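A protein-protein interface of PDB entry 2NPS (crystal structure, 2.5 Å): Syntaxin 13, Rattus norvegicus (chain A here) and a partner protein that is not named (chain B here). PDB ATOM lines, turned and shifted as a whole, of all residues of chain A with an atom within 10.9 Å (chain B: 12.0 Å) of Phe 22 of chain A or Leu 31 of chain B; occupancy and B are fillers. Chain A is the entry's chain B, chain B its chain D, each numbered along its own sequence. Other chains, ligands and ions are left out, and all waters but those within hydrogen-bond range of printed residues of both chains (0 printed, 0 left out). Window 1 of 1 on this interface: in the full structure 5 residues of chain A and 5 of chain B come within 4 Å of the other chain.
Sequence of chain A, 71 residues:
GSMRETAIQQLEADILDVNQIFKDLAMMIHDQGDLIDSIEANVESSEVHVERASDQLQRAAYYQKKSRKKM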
ATOM      1  N   ASP A  14       2.198 -16.118 -18.351  1.00  0.00           N
ATOM      2  CA  ASP A  14       2.656 -15.460 -19.556  1.00  0.00           C
ATOM      3  C   ASP A  14       3.420 -14.174 -19.257  1.00  0.00           C
ATOM      4  O   ASP A  14       4.320 -13.793 -20.002  1.00  0.00           O
ATOM      5  CB  ASP A  14       1.481 -15.215 -20.492  1.00  0.00           C
ATOM      6  CG  ASP A  14       1.077 -16.484 -21.244  1.00  0.00           C
ATOM      7  OD1 ASP A  14       0.095 -16.460 -22.022  1.00  0.00           O
ATOM      8  OD2 ASP A  14       1.760 -17.522 -21.056  1.00  0.00           O
ATOM      9  N   ILE A  15       3.092 -13.516 -18.151  1.00  0.00           N
ATOM     10  CA  ILE A  15       3.824 -12.312 -17.792  1.00  0.00           C
ATOM     11  C   ILE A  15       5.226 -12.723 -17.369  1.00  0.00           C
ATOM     12  O   ILE A  15       6.180 -11.974 -17.558  1.00  0.00           O
ATOM     13  CB  ILE A  15       3.154 -11.527 -16.642  1.00  0.00           C
ATOM     14  CG1 ILE A  15       1.901 -10.805 -17.166  1.00  0.00           C
ATOM     15  CG2 ILE A  15       4.143 -10.518 -16.061  1.00  0.00           C
ATOM     16  CD1 ILE A  15       1.170  -9.978 -16.110  1.00  0.00           C
ATOM     17  N   LEU A  16       5.358 -13.917 -16.802  1.00  0.00           N
ATOM     18  CA  LEU A  16       6.677 -14.393 -16.393  1.00  0.00           C
ATOM     19  C   LEU A  16       7.516 -14.678 -17.624  1.00  0.00           C
ATOM     20  O   LEU A  16       8.735 -14.569 -17.599  1.00  0.00           O
ATOM     21  CB  LEU A  16       6.573 -15.669 -15.559  1.00  0.00           C
ATOM     22  CG  LEU A  16       6.630 -15.443 -14.057  1.00  0.00           C
ATOM     23  CD1 LEU A  16       6.661 -16.787 -13.341  1.00  0.00           C
ATOM     24  CD2 LEU A  16       7.873 -14.643 -13.714  1.00  0.00           C
ATOM     25  N   ASP A  17       6.840 -15.064 -18.698  1.00  0.00           N
ATOM     26  CA  ASP A  17       7.498 -15.366 -19.955  1.00  0.00           C
ATOM     27  C   ASP A  17       8.164 -14.120 -20.486  1.00  0.00           C
ATOM     28  O   ASP A  17       9.338 -14.151 -20.837  1.00  0.00           O
ATOM     29  CB  ASP A  17       6.485 -15.873 -20.979  1.00  0.00           C
ATOM     30  CG  ASP A  17       6.313 -17.383 -20.929  1.00  0.00           C
ATOM     31  OD1 ASP A  17       6.724 -18.002 -19.918  1.00  0.00           O
ATOM     32  OD2 ASP A  17       5.757 -17.957 -21.896  1.00  0.00           O
ATOM     33  N   VAL A  18       7.417 -13.020 -20.544  1.00  0.00           N
ATOM     34  CA  VAL A  18       7.980 -11.783 -21.048  1.00  0.00           C
ATOM     35  C   VAL A  18       9.191 -11.440 -20.194  1.00  0.00           C
ATOM     36  O   VAL A  18      10.270 -11.172 -20.718  1.00  0.00           O
ATOM     37  CB  VAL A  18       6.953 -10.617 -21.029  1.00  0.00           C
ATOM     38  CG1 VAL A  18       5.633 -11.088 -21.580  1.00  0.00           C
ATOM     39  CG2 VAL A  18       6.770 -10.068 -19.633  1.00  0.00           C
ATOM     40  N   ASN A  19       9.030 -11.489 -18.876  1.00  0.00           N
ATOM     41  CA  ASN A  19      10.136 -11.163 -17.992  1.00  0.00           C
ATOM     42  C   ASN A  19      11.345 -12.006 -18.335  1.00  0.00           C
ATOM     43  O   ASN A  19      12.478 -11.529 -18.287  1.00  0.00           O
ATOM     44  CB  ASN A  19       9.752 -11.378 -16.531  1.00  0.00           C
ATOM     45  CG  ASN A  19      10.861 -10.965 -15.578  1.00  0.00           C
ATOM     46  OD1 ASN A  19      11.755 -11.751 -15.266  1.00  0.00           O
ATOM     47  ND2 ASN A  19      10.818  -9.719 -15.128  1.00  0.00           N
ATOM     48  N   GLN A  20      11.100 -13.258 -18.693  1.00  0.00           N
ATOM     49  CA  GLN A  20      12.189 -14.135 -19.046  1.00  0.00           C
ATOM     50  C   GLN A  20      12.789 -13.704 -20.380  1.00  0.00           C
ATOM     51  O   GLN A  20      13.998 -13.512 -20.487  1.00  0.00           O
ATOM     52  CB  GLN A  20      11.698 -15.585 -19.105  1.00  0.00           C
ATOM     53  CG  GLN A  20      12.805 -16.615 -19.332  1.00  0.00           C
ATOM     54  CD  GLN A  20      14.070 -16.299 -18.541  1.00  0.00           C
ATOM     55  OE1 GLN A  20      14.013 -16.029 -17.341  1.00  0.00           O
ATOM     56  NE2 GLN A  20      15.218 -16.334 -19.213  1.00  0.00           N
ATOM     57  N   ILE A  21      11.943 -13.525 -21.390  1.00  0.00           N
ATOM     58  CA  ILE A  21      12.426 -13.128 -22.700  1.00  0.00           C
ATOM     59  C   ILE A  21      13.184 -11.806 -22.617  1.00  0.00           C
ATOM     60  O   ILE A  21      14.171 -11.610 -23.315  1.00  0.00           O
ATOM     61  CB  ILE A  21      11.271 -12.996 -23.720  1.00  0.00           C
ATOM     62  CG1 ILE A  21      10.388 -14.244 -23.686  1.00  0.00           C
ATOM     63  CG2 ILE A  21      11.833 -12.877 -25.140  1.00  0.00           C
ATOM     64  N   PHE A  22      12.726 -10.893 -21.772  1.00  0.00           N
ATOM     65  CA  PHE A  22      13.422  -9.625 -21.630  1.00  0.00           C
ATOM     66  C   PHE A  22      14.794  -9.844 -21.010  1.00  0.00           C
ATOM     67  O   PHE A  22      15.773  -9.227 -21.421  1.00  0.00           O
ATOM     68  CB  PHE A  22      12.635  -8.653 -20.767  1.00  0.00           C
ATOM     69  CG  PHE A  22      11.692  -7.772 -21.540  1.00  0.00           C
ATOM     70  CD1 PHE A  22      10.604  -8.306 -22.209  1.00  0.00           C
ATOM     71  CD2 PHE A  22      11.880  -6.391 -21.569  1.00  0.00           C
ATOM     72  CE1 PHE A  22       9.713  -7.479 -22.881  1.00  0.00           C
ATOM     73  CE2 PHE A  22      10.998  -5.559 -22.236  1.00  0.00           C
ATOM     74  CZ  PHE A  22       9.912  -6.101 -22.899  1.00  0.00           C
ATOM     75  N   LYS A  23      14.881 -10.710 -20.008  1.00  0.00           N
ATOM     76  CA  LYS A  23      16.187 -10.981 -19.408  1.00  0.00           C
ATOM     77  C   LYS A  23      17.045 -11.604 -20.496  1.00  0.00           C
ATOM     78  O   LYS A  23      18.160 -11.156 -20.734  1.00  0.00           O
ATOM     79  CB  LYS A  23      16.070 -11.934 -18.215  1.00  0.00           C
ATOM     80  CG  LYS A  23      15.551 -11.271 -16.946  1.00  0.00           C
ATOM     81  CD  LYS A  23      15.424 -12.266 -15.798  1.00  0.00           C
ATOM     82  CE  LYS A  23      14.812 -11.616 -14.546  1.00  0.00           C
ATOM     83  NZ  LYS A  23      15.698 -10.556 -13.966  1.00  0.00           N
ATOM     84  N   ASP A  24      16.507 -12.613 -21.178  1.00  0.00           N
ATOM     85  CA  ASP A  24      17.228 -13.271 -22.262  1.00  0.00           C
ATOM     86  C   ASP A  24      17.788 -12.273 -23.272  1.00  0.00           C
ATOM     87  O   ASP A  24      18.965 -12.331 -23.618  1.00  0.00           O
ATOM     88  CB  ASP A  24      16.319 -14.263 -22.983  1.00  0.00           C
ATOM     89  CG  ASP A  24      16.196 -15.598 -22.247  1.00  0.00           C
ATOM     90  OD1 ASP A  24      16.844 -15.792 -21.185  1.00  0.00           O
ATOM     91  OD2 ASP A  24      15.440 -16.463 -22.750  1.00  0.00           O
ATOM     92  N   LEU A  25      16.949 -11.355 -23.738  1.00  0.00           N
ATOM     93  CA  LEU A  25      17.389 -10.377 -24.720  1.00  0.00           C
ATOM     94  C   LEU A  25      18.488  -9.491 -24.161  1.00  0.00           C
ATOM     95  O   LEU A  25      19.508  -9.275 -24.808  1.00  0.00           O
ATOM     96  CB  LEU A  25      16.213  -9.518 -25.176  1.00  0.00           C
ATOM     97  CG  LEU A  25      16.424  -8.699 -26.449  1.00  0.00           C
ATOM     98  CD1 LEU A  25      16.545  -9.631 -27.658  1.00  0.00           C
ATOM     99  CD2 LEU A  25      15.263  -7.729 -26.645  1.00  0.00           C
ATOM    100  N   ALA A  26      18.275  -8.985 -22.951  1.00  0.00           N
ATOM    101  CA  ALA A  26      19.248  -8.120 -22.296  1.00  0.00           C
ATOM    102  C   ALA A  26      20.599  -8.817 -22.209  1.00  0.00           C
ATOM    103  O   ALA A  26      21.634  -8.228 -22.504  1.00  0.00           O
ATOM    104  CB  ALA A  26      18.763  -7.749 -20.902  1.00  0.00           C
ATOM    105  N   MET A  27      20.577 -10.079 -21.800  1.00  0.00           N
ATOM    106  CA  MET A  27      21.782 -10.894 -21.667  1.00  0.00           C
ATOM    107  C   MET A  27      22.501 -11.002 -23.012  1.00  0.00           C
ATOM    108  O   MET A  27      23.700 -10.767 -23.100  1.00  0.00           O
ATOM    109  CB  MET A  27      21.379 -12.277 -21.158  1.00  0.00           C
ATOM    110  CG  MET A  27      22.415 -13.359 -21.276  1.00  0.00           C
ATOM    111  SD  MET A  27      21.602 -14.960 -21.088  1.00  0.00           S
ATOM    112  CE  MET A  27      21.130 -15.277 -22.823  1.00  0.00           C
ATOM    113  N   MET A  28      21.760 -11.348 -24.062  1.00  0.00           N
ATOM    114  CA  MET A  28      22.342 -11.470 -25.388  1.00  0.00           C
ATOM    115  C   MET A  28      23.004 -10.185 -25.857  1.00  0.00           C
ATOM    116  O   MET A  28      24.120 -10.212 -26.376  1.00  0.00           O
ATOM    117  CB  MET A  28      21.280 -11.870 -26.391  1.00  0.00           C
ATOM    118  CG  MET A  28      20.765 -13.269 -26.218  1.00  0.00           C
ATOM    119  SD  MET A  28      19.847 -13.777 -27.667  1.00  0.00           S
ATOM    120  CE  MET A  28      18.305 -12.926 -27.371  1.00  0.00           C
ATOM    121  N   ILE A  29      22.311  -9.066 -25.676  1.00  0.00           N
ATOM    122  CA  ILE A  29      22.829  -7.774 -26.083  1.00  0.00           C
ATOM    123  C   ILE A  29      24.078  -7.432 -25.285  1.00  0.00           C
ATOM    124  O   ILE A  29      25.055  -6.917 -25.822  1.00  0.00           O
ATOM    125  CB  ILE A  29      21.759  -6.666 -25.901  1.00  0.00           C
ATOM    126  CG1 ILE A  29      20.619  -6.880 -26.898  1.00  0.00           C
ATOM    127  CG2 ILE A  29      22.380  -5.271 -26.103  1.00  0.00           C
ATOM    128  CD1 ILE A  29      19.506  -5.877 -26.791  1.00  0.00           C
ATOM    129  N   HIS A  30      24.059  -7.732 -23.996  1.00  0.00           N
ATOM    130  CA  HIS A  30      25.211  -7.429 -23.159  1.00  0.00           C
ATOM    131  C   HIS A  30      26.441  -8.238 -23.530  1.00  0.00           C
ATOM    132  O   HIS A  30      27.555  -7.731 -23.499  1.00  0.00           O
ATOM    133  CB  HIS A  30      24.873  -7.651 -21.687  1.00  0.00           C
ATOM    134  CG  HIS A  30      26.053  -7.531 -20.777  1.00  0.00           C
ATOM    135  ND1 HIS A  30      26.989  -8.538 -20.638  1.00  0.00           N
ATOM    136  CD2 HIS A  30      26.476  -6.513 -19.991  1.00  0.00           C
ATOM    137  CE1 HIS A  30      27.937  -8.142 -19.806  1.00  0.00           C
ATOM    138  NE2 HIS A  30      27.648  -6.917 -19.400  1.00  0.00           N
ATOM    139  N   ASP A  31      26.238  -9.497 -23.886  1.00  0.00           N
ATOM    140  CA  ASP A  31      27.347 -10.358 -24.248  1.00  0.00           C
ATOM    141  C   ASP A  31      27.985  -9.974 -25.579  1.00  0.00           C
ATOM    142  O   ASP A  31      29.169 -10.208 -25.801  1.00  0.00           O
ATOM    143  CB  ASP A  31      26.869 -11.815 -24.278  1.00  0.00           C
ATOM    144  CG  ASP A  31      26.504 -12.342 -22.892  1.00  0.00           C
ATOM    145  OD1 ASP A  31      25.732 -13.324 -22.804  1.00  0.00           O
ATOM    146  OD2 ASP A  31      27.005 -11.778 -21.887  1.00  0.00           O
ATOM    147  N   GLU B  22      -5.956  -3.300 -14.553  1.00  0.00           N
ATOM    148  CA  GLU B  22      -5.793  -2.056 -15.279  1.00  0.00           C
ATOM    149  C   GLU B  22      -4.325  -1.692 -15.086  1.00  0.00           C
ATOM    150  O   GLU B  22      -3.659  -1.258 -16.019  1.00  0.00           O
ATOM    151  CB  GLU B  22      -6.713  -0.983 -14.677  1.00  0.00           C
ATOM    152  CG  GLU B  22      -6.865   0.299 -15.485  1.00  0.00           C
ATOM    153  CD  GLU B  22      -7.460   0.061 -16.865  1.00  0.00           C
ATOM    154  OE1 GLU B  22      -8.388  -0.778 -16.965  1.00  0.00           O
ATOM    155  OE2 GLU B  22      -7.014   0.723 -17.839  1.00  0.00           O
ATOM    156  N   LEU B  23      -3.831  -1.896 -13.864  1.00  0.00           N
ATOM    157  CA  LEU B  23      -2.433  -1.628 -13.506  1.00  0.00           C
ATOM    158  C   LEU B  23      -1.493  -2.578 -14.256  1.00  0.00           C
ATOM    159  O   LEU B  23      -0.352  -2.238 -14.564  1.00  0.00           O
ATOM    160  CB  LEU B  23      -2.222  -1.794 -11.990  1.00  0.00           C
ATOM    161  CG  LEU B  23      -2.779  -0.742 -11.031  1.00  0.00           C
ATOM    162  N   VAL B  24      -1.990  -3.778 -14.534  1.00  0.00           N
ATOM    163  CA  VAL B  24      -1.210  -4.770 -15.262  1.00  0.00           C
ATOM    164  C   VAL B  24      -1.233  -4.385 -16.727  1.00  0.00           C
ATOM    165  O   VAL B  24      -0.202  -4.395 -17.396  1.00  0.00           O
ATOM    166  CB  VAL B  24      -1.790  -6.196 -15.096  1.00  0.00           C
ATOM    167  CG1 VAL B  24      -1.350  -7.077 -16.245  1.00  0.00           C
ATOM    168  CG2 VAL B  24      -1.327  -6.799 -13.767  1.00  0.00           C
ATOM    169  N   SER B  25      -2.412  -4.023 -17.218  1.00  0.00           N
ATOM    170  CA  SER B  25      -2.567  -3.630 -18.612  1.00  0.00           C
ATOM    171  C   SER B  25      -1.740  -2.412 -18.958  1.00  0.00           C
ATOM    172  O   SER B  25      -1.256  -2.274 -20.082  1.00  0.00           O
ATOM    173  CB  SER B  25      -4.020  -3.319 -18.928  1.00  0.00           C
ATOM    174  OG  SER B  25      -4.106  -2.641 -20.172  1.00  0.00           O
ATOM    175  N   GLY B  26      -1.594  -1.515 -17.994  1.00  0.00           N
ATOM    176  CA  GLY B  26      -0.806  -0.329 -18.246  1.00  0.00           C
ATOM    177  C   GLY B  26       0.638  -0.769 -18.315  1.00  0.00           C
ATOM    178  O   GLY B  26       1.329  -0.545 -19.309  1.00  0.00           O
ATOM    179  N   SER B  27       1.085  -1.415 -17.244  1.00  0.00           N
ATOM    180  CA  SER B  27       2.454  -1.894 -17.150  1.00  0.00           C
ATOM    181  C   SER B  27       2.884  -2.630 -18.402  1.00  0.00           C
ATOM    182  O   SER B  27       3.954  -2.368 -18.947  1.00  0.00           O
ATOM    183  CB  SER B  27       2.611  -2.824 -15.946  1.00  0.00           C
ATOM    184  OG  SER B  27       3.903  -3.423 -15.935  1.00  0.00           O
ATOM    185  N   ILE B  28       2.045  -3.554 -18.854  1.00  0.00           N
ATOM    186  CA  ILE B  28       2.352  -4.333 -20.040  1.00  0.00           C
ATOM    187  C   ILE B  28       2.420  -3.466 -21.284  1.00  0.00           C
ATOM    188  O   ILE B  28       3.308  -3.634 -22.116  1.00  0.00           O
ATOM    189  CB  ILE B  28       1.318  -5.427 -20.279  1.00  0.00           C
ATOM    190  CG1 ILE B  28       1.609  -6.122 -21.603  1.00  0.00           C
ATOM    191  CG2 ILE B  28      -0.059  -4.830 -20.332  1.00  0.00           C
ATOM    192  N   GLY B  29       1.470  -2.545 -21.411  1.00  0.00           N
ATOM    193  CA  GLY B  29       1.446  -1.662 -22.560  1.00  0.00           C
ATOM    194  C   GLY B  29       2.825  -1.090 -22.807  1.00  0.00           C
ATOM    195  O   GLY B  29       3.321  -1.095 -23.932  1.00  0.00           O
ATOM    196  N   VAL B  30       3.441  -0.595 -21.736  1.00  0.00           N
ATOM    197  CA  VAL B  30       4.782  -0.019 -21.803  1.00  0.00           C
ATOM    198  C   VAL B  30       5.763  -1.063 -22.337  1.00  0.00           C
ATOM    199  O   VAL B  30       6.578  -0.778 -23.222  1.00  0.00           O
ATOM    200  CB  VAL B  30       5.262   0.444 -20.412  1.00  0.00           C
ATOM    201  CG1 VAL B  30       6.715   0.900 -20.478  1.00  0.00           C
ATOM    202  CG2 VAL B  30       4.381   1.573 -19.920  1.00  0.00           C
ATOM    203  N   LEU B  31       5.683  -2.274 -21.794  1.00  0.00           N
ATOM    204  CA  LEU B  31       6.548  -3.361 -22.233  1.00  0.00           C
ATOM    205  C   LEU B  31       6.321  -3.524 -23.721  1.00  0.00           C
ATOM    206  O   LEU B  31       7.253  -3.774 -24.480  1.00  0.00           O
ATOM    207  CB  LEU B  31       6.188  -4.664 -21.515  1.00  0.00           C
ATOM    208  CG  LEU B  31       6.423  -4.696 -20.008  1.00  0.00           C
ATOM    209  N   LYS B  32       5.064  -3.380 -24.128  1.00  0.00           N
ATOM    210  CA  LYS B  32       4.694  -3.484 -25.532  1.00  0.00           C
ATOM    211  C   LYS B  32       5.304  -2.311 -26.281  1.00  0.00           C
ATOM    212  O   LYS B  32       5.495  -2.368 -27.490  1.00  0.00           O
ATOM    213  CB  LYS B  32       3.175  -3.451 -25.691  1.00  0.00           C
ATOM    214  CG  LYS B  32       2.717  -3.362 -27.133  1.00  0.00           C
ATOM    215  N   ASN B  33       5.596  -1.239 -25.553  1.00  0.00           N
ATOM    216  CA  ASN B  33       6.199  -0.060 -26.156  1.00  0.00           C
ATOM    217  C   ASN B  33       7.687  -0.271 -26.258  1.00  0.00           C
ATOM    218  O   ASN B  33       8.277  -0.092 -27.320  1.00  0.00           O
ATOM    219  CB  ASN B  33       5.946   1.192 -25.314  1.00  0.00           C
ATOM    220  CG  ASN B  33       6.718   2.398 -25.823  1.00  0.00           C
ATOM    221  OD1 ASN B  33       7.728   2.808 -25.234  1.00  0.00           O
ATOM    222  ND2 ASN B  33       6.249   2.968 -26.932  1.00  0.00           N
ATOM    223  N   MET B  34       8.289  -0.646 -25.137  1.00  0.00           N
ATOM    224  CA  MET B  34       9.722  -0.863 -25.079  1.00  0.00           C
ATOM    225  C   MET B  34      10.178  -1.954 -26.020  1.00  0.00           C
ATOM    226  O   MET B  34      11.238  -1.848 -26.614  1.00  0.00           O
ATOM    227  CB  MET B  34      10.155  -1.214 -23.656  1.00  0.00           C
ATOM    228  CG  MET B  34      10.157  -0.052 -22.683  1.00  0.00           C
ATOM    229  SD  MET B  34      10.701  -0.568 -21.023  1.00  0.00           S
ATOM    230  CE  MET B  34      10.382   0.910 -20.103  1.00  0.00           C
ATOM    231  N   SER B  35       9.384  -3.005 -26.162  1.00  0.00           N
ATOM    232  CA  SER B  35       9.785  -4.083 -27.043  1.00  0.00           C
ATOM    233  C   SER B  35       9.897  -3.600 -28.484  1.00  0.00           C
ATOM    234  O   SER B  35      10.831  -3.960 -29.193  1.00  0.00           O
ATOM    235  CB  SER B  35       8.810  -5.262 -26.950  1.00  0.00           C
ATOM    236  OG  SER B  35       7.539  -4.933 -27.467  1.00  0.00           O
ATOM    237  N   GLN B  36       8.966  -2.759 -28.916  1.00  0.00           N
ATOM    238  CA  GLN B  36       8.994  -2.256 -30.289  1.00  0.00           C
ATOM    239  C   GLN B  36      10.133  -1.288 -30.584  1.00  0.00           C
ATOM    240  O   GLN B  36      10.767  -1.373 -31.630  1.00  0.00           O
ATOM    241  CB  GLN B  36       7.665  -1.596 -30.637  1.00  0.00           C
ATOM    242  CG  GLN B  36       6.472  -2.478 -30.398  1.00  0.00           C
ATOM    243  CD  GLN B  36       5.213  -1.885 -30.963  1.00  0.00           C
ATOM    244  OE1 GLN B  36       5.050  -1.807 -32.185  1.00  0.00           O
ATOM    245  NE2 GLN B  36       4.310  -1.448 -30.083  1.00  0.00           N
ATOM    246  N   ARG B  37      10.387  -0.355 -29.678  1.00  0.00           N
ATOM    247  CA  ARG B  37      11.477   0.588 -29.875  1.00  0.00           C
ATOM    248  C   ARG B  37      12.799  -0.187 -29.971  1.00  0.00           C
ATOM    249  O   ARG B  37      13.739   0.244 -30.635  1.00  0.00           O
ATOM    250  CB  ARG B  37      11.527   1.581 -28.714  1.00  0.00           C
ATOM    251  CG  ARG B  37      10.335   2.544 -28.663  1.00  0.00           C
ATOM    252  CD  ARG B  37      10.119   3.106 -27.258  1.00  0.00           C
ATOM    253  NE  ARG B  37      11.332   3.699 -26.700  1.00  0.00           N
ATOM    254  CZ  ARG B  37      11.537   3.891 -25.400  1.00  0.00           C
ATOM    255  NH1 ARG B  37      12.666   4.441 -24.976  1.00  0.00           N
ATOM    256  NH2 ARG B  37      10.616   3.527 -24.511  1.00  0.00           N
ATOM    257  N   ILE B  38      12.842  -1.336 -29.296  1.00  0.00           N
ATOM    258  CA  ILE B  38      13.993  -2.229 -29.271  1.00  0.00           C
ATOM    259  C   ILE B  38      14.133  -2.883 -30.629  1.00  0.00           C
ATOM    260  O   ILE B  38      15.232  -2.994 -31.165  1.00  0.00           O
ATOM    261  CB  ILE B  38      13.803  -3.342 -28.220  1.00  0.00           C
ATOM    262  CG1 ILE B  38      13.866  -2.742 -26.813  1.00  0.00           C
ATOM    263  CG2 ILE B  38      14.845  -4.434 -28.416  1.00  0.00           C
ATOM    264  CD1 ILE B  38      13.427  -3.698 -25.721  1.00  0.00           C
ATOM    265  N   GLY B  39      13.009  -3.329 -31.173  1.00  0.00           N
ATOM    266  CA  GLY B  39      13.021  -3.960 -32.477  1.00  0.00           C
ATOM    267  C   GLY B  39      13.395  -2.958 -33.553  1.00  0.00           C
ATOM    268  O   GLY B  39      14.094  -3.299 -34.514  1.00  0.00           O
ATOM    269  N   GLY B  40      12.931  -1.718 -33.383  1.00  0.00           N
ATOM    270  CA  GLY B  40      13.228  -0.666 -34.338  1.00  0.00           C
ATOM    271  C   GLY B  40      14.707  -0.343 -34.338  1.00  0.00           C
ATOM    272  O   GLY B  40      15.354  -0.281 -35.394  1.00  0.00           O
ATOM    273  N   LEU B  42      17.056  -2.241 -33.212  1.00  0.00           N
ATOM    274  CA  LEU B  42      17.815  -3.392 -33.674  1.00  0.00           C
ATOM    275  C   LEU B  42      17.832  -3.436 -35.194  1.00  0.00           C
ATOM    276  O   LEU B  42      18.831  -3.803 -35.801  1.00  0.00           O
ATOM    277  CB  LEU B  42      17.222  -4.686 -33.115  1.00  0.00           C
ATOM    278  CG  LEU B  42      17.495  -4.947 -31.633  1.00  0.00           C
ATOM    279  CD1 LEU B  42      16.667  -6.120 -31.127  1.00  0.00           C
ATOM    280  CD2 LEU B  42      18.972  -5.216 -31.441  1.00  0.00           C
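Of the 18 printed residues of chain A, 3 touch a printed residue of chain B.
Hydrophobic or aromatic side chains of chain A within 4 Å of the printed part of chain B: Ile 15, Phe 22 and Leu 25.
Of the 20 printed residues of chain B, 3 touch a printed residue of chain A.
Along chain B the printed residues that touch a printed residue of chain A span positions 24 to 38.
Among the printed residues, merely in contact across the chains: Ile 15 of chain A with Val 24 of chain B (3.8 Å), Phe 22 of chain A with Leu 31 of chain B (3.9 Å) and Leu 25 of chain A with Ile 38 of chain B (3.8 Å).
The side-chain hydroxyl of Ser 35 of chain B is in hydrogen-bond range of the backbone carbonyl oxygen of Leu 31 of chain B.
Printed residues of chain B within 4 Å of Ile 15 of chain A: Val 24 (3.8 Å).
No residue of chain B comes within 4 Å of Val 18 of chain A.
No residue of chain B comes within 4 Å of Asn 19 of chain A.
No residue of chain B comes within 4 Å of Gln 20 of chain A.
No residue of chain B comes within 4 Å of Ile 21 of chain A.
Phe 22 of chain A touches just one residue of chain B: Leu 31 (3.9 Å).
No residue of chain B comes within 4 Å of Lys 23 of chain A.
No residue of chain B comes within 4 Å of Asp 24 of chain A.
No residue of chain B comes within 4 Å of Ala 26 of chain A.
Of the printed residues of chain A, Val 24 of chain B touches Ile 15.
No residue of chain A comes within 4 Å of Ile 28 of chain B.
No residue of chain A comes within 4 Å of Gly 29 of chain B.
Val 30 of chain B touches none of the printed residues of chain A.
No residue of chain A comes within 4 Å of Ser 35 of chain B.
Of the printed residues of chain A, Ile 38 of chain B touches Leu 25 (3.8 Å).
The nearest residue of chain B that does not touch Phe 22 of chain A is Ser 35 of chain B (4.3 Å).
The nearest residue of chain A that does not touch Leu 31 of chain B is Val 18 of chain A (5.4 Å).
The nearest printed residue of chain A that does not touch Val 24 of chain B is Asp 14 of chain A (9.1 Å).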
